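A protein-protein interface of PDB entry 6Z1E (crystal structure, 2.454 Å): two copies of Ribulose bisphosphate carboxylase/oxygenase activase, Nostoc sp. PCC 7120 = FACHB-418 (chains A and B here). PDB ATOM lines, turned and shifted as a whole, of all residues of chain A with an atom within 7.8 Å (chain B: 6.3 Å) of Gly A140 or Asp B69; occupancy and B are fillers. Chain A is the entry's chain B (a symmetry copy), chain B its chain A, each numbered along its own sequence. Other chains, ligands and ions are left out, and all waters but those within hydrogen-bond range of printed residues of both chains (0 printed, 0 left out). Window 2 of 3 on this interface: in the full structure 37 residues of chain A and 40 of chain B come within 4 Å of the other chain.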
ATOM      1  N   ARG A  78      19.646 -26.765 -26.122  1.00  0.00           N
ATOM      2  CA  ARG A  78      20.053 -25.661 -25.264  1.00  0.00           C
ATOM      3  C   ARG A  78      21.570 -25.475 -25.255  1.00  0.00           C
ATOM      4  O   ARG A  78      22.054 -24.345 -25.219  1.00  0.00           O
ATOM      5  CB  ARG A  78      19.517 -25.871 -23.847  1.00  0.00           C
ATOM      6  CG  ARG A  78      18.008 -25.713 -23.761  1.00  0.00           C
ATOM      7  CD  ARG A  78      17.485 -26.132 -22.405  1.00  0.00           C
ATOM      8  NE  ARG A  78      16.086 -25.756 -22.211  1.00  0.00           N
ATOM      9  CZ  ARG A  78      15.662 -24.520 -21.961  1.00  0.00           C
ATOM     10  NH1 ARG A  78      16.525 -23.515 -21.888  1.00  0.00           N
ATOM     11  NH2 ARG A  78      14.369 -24.287 -21.788  1.00  0.00           N
ATOM     12  N   GLN A 137      18.882 -21.211 -20.147  1.00  0.00           N
ATOM     13  CA  GLN A 137      19.718 -21.983 -19.243  1.00  0.00           C
ATOM     14  C   GLN A 137      19.680 -23.457 -19.610  1.00  0.00           C
ATOM     15  O   GLN A 137      18.728 -23.920 -20.238  1.00  0.00           O
ATOM     16  CB  GLN A 137      19.223 -21.804 -17.811  1.00  0.00           C
ATOM     17  CG  GLN A 137      19.102 -20.354 -17.374  1.00  0.00           C
ATOM     18  CD  GLN A 137      20.448 -19.659 -17.283  1.00  0.00           C
ATOM     19  OE1 GLN A 137      21.483 -20.304 -17.116  1.00  0.00           O
ATOM     20  NE2 GLN A 137      20.439 -18.334 -17.392  1.00  0.00           N
ATOM     21  N   LEU A 138      20.719 -24.188 -19.220  1.00  0.00           N
ATOM     22  CA  LEU A 138      20.712 -25.638 -19.333  1.00  0.00           C
ATOM     23  C   LEU A 138      19.864 -26.196 -18.202  1.00  0.00           C
ATOM     24  O   LEU A 138      19.779 -25.579 -17.140  1.00  0.00           O
ATOM     25  CB  LEU A 138      22.125 -26.200 -19.216  1.00  0.00           C
ATOM     26  CG  LEU A 138      23.157 -25.769 -20.254  1.00  0.00           C
ATOM     27  CD1 LEU A 138      24.488 -26.433 -19.939  1.00  0.00           C
ATOM     28  CD2 LEU A 138      22.694 -26.126 -21.653  1.00  0.00           C
ATOM     29  N   PRO A 139      19.244 -27.368 -18.414  1.00  0.00           N
ATOM     30  CA  PRO A 139      18.457 -27.952 -17.324  1.00  0.00           C
ATOM     31  C   PRO A 139      19.292 -28.163 -16.065  1.00  0.00           C
ATOM     32  O   PRO A 139      20.313 -28.849 -16.113  1.00  0.00           O
ATOM     33  CB  PRO A 139      17.997 -29.296 -17.901  1.00  0.00           C
ATOM     34  CG  PRO A 139      18.067 -29.129 -19.378  1.00  0.00           C
ATOM     35  CD  PRO A 139      19.222 -28.210 -19.624  1.00  0.00           C
ATOM     36  N   GLY A 140      18.866 -27.561 -14.960  1.00  0.00           N
ATOM     37  CA  GLY A 140      19.545 -27.717 -13.686  1.00  0.00           C
ATOM     38  C   GLY A 140      20.492 -26.571 -13.385  1.00  0.00           C
ATOM     39  O   GLY A 140      20.919 -26.396 -12.242  1.00  0.00           O
ATOM     40  N   SER A 141      20.817 -25.788 -14.410  1.00  0.00           N
ATOM     41  CA  SER A 141      21.753 -24.679 -14.266  1.00  0.00           C
ATOM     42  C   SER A 141      21.023 -23.343 -14.253  1.00  0.00           C
ATOM     43  O   SER A 141      19.927 -23.221 -14.801  1.00  0.00           O
ATOM     44  CB  SER A 141      22.758 -24.700 -15.418  1.00  0.00           C
ATOM     45  OG  SER A 141      23.485 -25.915 -15.434  1.00  0.00           O
ATOM     46  N   TYR A 142      21.632 -22.348 -13.615  1.00  0.00           N
ATOM     47  CA  TYR A 142      21.133 -20.980 -13.687  1.00  0.00           C
ATOM     48  C   TYR A 142      22.272 -19.973 -13.722  1.00  0.00           C
ATOM     49  O   TYR A 142      23.233 -20.067 -12.960  1.00  0.00           O
ATOM     50  CB  TYR A 142      20.193 -20.654 -12.526  1.00  0.00           C
ATOM     51  CG  TYR A 142      19.553 -19.295 -12.692  1.00  0.00           C
ATOM     52  CD1 TYR A 142      18.472 -19.119 -13.542  1.00  0.00           C
ATOM     53  CD2 TYR A 142      20.045 -18.185 -12.018  1.00  0.00           C
ATOM     54  CE1 TYR A 142      17.890 -17.879 -13.712  1.00  0.00           C
ATOM     55  CE2 TYR A 142      19.471 -16.940 -12.180  1.00  0.00           C
ATOM     56  CZ  TYR A 142      18.395 -16.792 -13.029  1.00  0.00           C
ATOM     57  OH  TYR A 142      17.813 -15.556 -13.195  1.00  0.00           O
ATOM     58  N   ASP A 143      22.129 -18.998 -14.612  1.00  0.00           N
ATOM     59  CA  ASP A 143      23.155 -18.003 -14.880  1.00  0.00           C
ATOM     60  C   ASP A 143      22.468 -16.656 -15.036  1.00  0.00           C
ATOM     61  O   ASP A 143      21.617 -16.487 -15.904  1.00  0.00           O
ATOM     62  CB  ASP A 143      23.890 -18.366 -16.170  1.00  0.00           C
ATOM     63  CG  ASP A 143      25.101 -17.484 -16.433  1.00  0.00           C
ATOM     64  OD1 ASP A 143      25.300 -16.496 -15.693  1.00  0.00           O
ATOM     65  OD2 ASP A 143      25.849 -17.775 -17.389  1.00  0.00           O
ATOM     66  N   GLU B  64      15.014 -20.245 -11.751  1.00  0.00           N
ATOM     67  CA  GLU B  64      15.921 -20.126 -10.621  1.00  0.00           C
ATOM     68  C   GLU B  64      15.546 -21.143  -9.549  1.00  0.00           C
ATOM     69  O   GLU B  64      16.411 -21.806  -8.982  1.00  0.00           O
ATOM     70  CB  GLU B  64      15.863 -18.712 -10.045  1.00  0.00           C
ATOM     71  CG  GLU B  64      17.134 -18.272  -9.341  1.00  0.00           C
ATOM     72  CD  GLU B  64      17.169 -16.777  -9.076  1.00  0.00           C
ATOM     73  OE1 GLU B  64      16.199 -16.082  -9.450  1.00  0.00           O
ATOM     74  OE2 GLU B  64      18.171 -16.298  -8.502  1.00  0.00           O
ATOM     75  N   GLU B  66      14.022 -23.806 -10.090  1.00  0.00           N
ATOM     76  CA  GLU B  66      14.141 -25.123 -10.699  1.00  0.00           C
ATOM     77  C   GLU B  66      15.572 -25.641 -10.595  1.00  0.00           C
ATOM     78  O   GLU B  66      15.806 -26.851 -10.618  1.00  0.00           O
ATOM     79  CB  GLU B  66      13.724 -25.060 -12.172  1.00  0.00           C
ATOM     80  CG  GLU B  66      13.466 -26.419 -12.809  1.00  0.00           C
ATOM     81  CD  GLU B  66      13.079 -26.310 -14.272  1.00  0.00           C
ATOM     82  OE1 GLU B  66      13.969 -26.034 -15.105  1.00  0.00           O
ATOM     83  OE2 GLU B  66      11.884 -26.497 -14.585  1.00  0.00           O
ATOM     84  N   SER B  67      16.523 -24.720 -10.473  1.00  0.00           N
ATOM     85  CA  SER B  67      17.940 -25.061 -10.535  1.00  0.00           C
ATOM     86  C   SER B  67      18.549 -25.338  -9.156  1.00  0.00           C
ATOM     87  O   SER B  67      18.441 -24.511  -8.250  1.00  0.00           O
ATOM     88  CB  SER B  67      18.720 -23.933 -11.209  1.00  0.00           C
ATOM     89  OG  SER B  67      20.101 -24.246 -11.279  1.00  0.00           O
ATOM     90  N   PRO B  68      19.197 -26.506  -8.993  1.00  0.00           N
ATOM     91  CA  PRO B  68      19.987 -26.781  -7.787  1.00  0.00           C
ATOM     92  C   PRO B  68      21.049 -25.717  -7.515  1.00  0.00           C
ATOM     93  O   PRO B  68      21.482 -25.568  -6.370  1.00  0.00           O
ATOM     94  CB  PRO B  68      20.656 -28.115  -8.114  1.00  0.00           C
ATOM     95  CG  PRO B  68      19.705 -28.791  -9.020  1.00  0.00           C
ATOM     96  CD  PRO B  68      19.042 -27.711  -9.826  1.00  0.00           C
ATOM     97  N   ASP B  69      21.469 -24.994  -8.550  1.00  0.00           N
ATOM     98  CA  ASP B  69      22.439 -23.914  -8.378  1.00  0.00           C
ATOM     99  C   ASP B  69      21.874 -22.804  -7.500  1.00  0.00           C
ATOM    100  O   ASP B  69      22.623 -21.985  -6.971  1.00  0.00           O
ATOM    101  CB  ASP B  69      22.868 -23.340  -9.728  1.00  0.00           C
ATOM    102  CG  ASP B  69      23.822 -24.249 -10.474  1.00  0.00           C
ATOM    103  OD1 ASP B  69      24.067 -25.379 -10.000  1.00  0.00           O
ATOM    104  OD2 ASP B  69      24.324 -23.830 -11.539  1.00  0.00           O
ATOM    105  N   ALA B  70      20.554 -22.781  -7.351  1.00  0.00           N
ATOM    106  CA  ALA B  70      19.900 -21.866  -6.419  1.00  0.00           C
ATOM    107  C   ALA B  70      19.957 -22.431  -5.005  1.00  0.00           C
ATOM    108  O   ALA B  70      19.432 -21.827  -4.067  1.00  0.00           O
ATOM    109  CB  ALA B  70      18.458 -21.633  -6.828  1.00  0.00           C
ATOM    110  N   GLY B  71      20.592 -23.590  -4.855  1.00  0.00           N
ATOM    111  CA  GLY B  71      20.669 -24.251  -3.568  1.00  0.00           C
ATOM    112  C   GLY B  71      19.292 -24.679  -3.110  1.00  0.00           C
ATOM    113  O   GLY B  71      18.551 -25.327  -3.852  1.00  0.00           O
ATOM    114  N   THR B 113      13.165 -33.499 -18.625  1.00  0.00           N
ATOM    115  CA  THR B 113      14.459 -33.562 -17.958  1.00  0.00           C
ATOM    116  C   THR B 113      14.273 -33.942 -16.497  1.00  0.00           C
ATOM    117  O   THR B 113      13.150 -33.987 -15.994  1.00  0.00           O
ATOM    118  CB  THR B 113      15.187 -32.212 -18.010  1.00  0.00           C
ATOM    119  OG1 THR B 113      14.419 -31.228 -17.308  1.00  0.00           O
ATOM    120  CG2 THR B 113      15.394 -31.762 -19.450  1.00  0.00           C
ATOM    121  N   TYR B 115      15.218 -32.238 -13.926  1.00  0.00           N
ATOM    122  CA  TYR B 115      15.018 -31.069 -13.074  1.00  0.00           C
ATOM    123  C   TYR B 115      13.647 -30.424 -13.236  1.00  0.00           C
ATOM    124  O   TYR B 115      13.217 -30.114 -14.346  1.00  0.00           O
ATOM    125  CB  TYR B 115      16.098 -30.029 -13.367  1.00  0.00           C
ATOM    126  CG  TYR B 115      17.485 -30.621 -13.440  1.00  0.00           C
ATOM    127  CD1 TYR B 115      18.247 -30.801 -12.294  1.00  0.00           C
ATOM    128  CD2 TYR B 115      18.032 -31.009 -14.656  1.00  0.00           C
ATOM    129  CE1 TYR B 115      19.515 -31.345 -12.355  1.00  0.00           C
ATOM    130  CE2 TYR B 115      19.298 -31.553 -14.728  1.00  0.00           C
ATOM    131  CZ  TYR B 115      20.036 -31.720 -13.575  1.00  0.00           C
ATOM    132  OH  TYR B 115      21.298 -32.262 -13.644  1.00  0.00           O
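The side-chain hydroxyl of Ser B67 sits at hydrogen-bond distance from the backbone carbonyl oxygen of Gly A140 (2.5 Å).
N of Tyr A142 lies within hydrogen-bond range of OG of Ser B67, at 3.4 Å.
OG1 of Thr B113 lies within hydrogen-bond range of O of Tyr B115 (3.4 Å).
N of Asp B69 sits close to OG of Ser B67 (3.1 Å).
Among the printed residues, merely in contact across the chains: Pro A139 with Tyr B115 (3.2 Å), Ser A141 with Ser B67 (3.2 Å), Gly A140 with Pro B68 (3.3 Å), Gly A140 with Tyr B115 (3.6 Å), Tyr A142 with Asp B69 (3.7 Å), Pro A139 with Thr B113 (3.8 Å), Ser A141 with Asp B69 (3.8 Å), Tyr A142 with Glu B64 (3.9 Å) and Gly A140 with Asp B69 (3.99 Å).
Of the printed residues of chain B, Gly A140 touches Ser B67 (2.5 Å), Pro B68 (3.3 Å), Asp B69 (3.99 Å) and Tyr B115 (3.6 Å).
Printed residues of chain A within 4 Å of Asp B69: Gly A140, Ser A141 and Tyr A142.
Of the printed residues of chain A, Ser B67 touches Gly A140, Ser A141 and Tyr A142.
Of the printed residues of chain A, Pro B68 touches Gly A140.
Of the printed residues of chain A, Glu B64 touches Tyr A142 (3.9 Å).
Ala B70 touches none of the printed residues of chain A.
The nearest printed residue of chain B that does not touch Gly A140 is Glu B66 (4.9 Å).
The nearest printed residue of chain A that does not touch Asp B69 is Asp A143 (6.1 Å).
Printed residues of chain A that touch a printed residue of chain B: Pro A139, Gly A140, Ser A141 and Tyr A142.
Along chain B the printed residues that touch a printed residue of chain A span positions 64 to 115.
Among the printed residues, 11 pairs touch across the chains.
No position is printed for both chains.
Of the 11 pairs that touch across the chains among the printed residues, none has its exchanged pair printed and touching as well.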
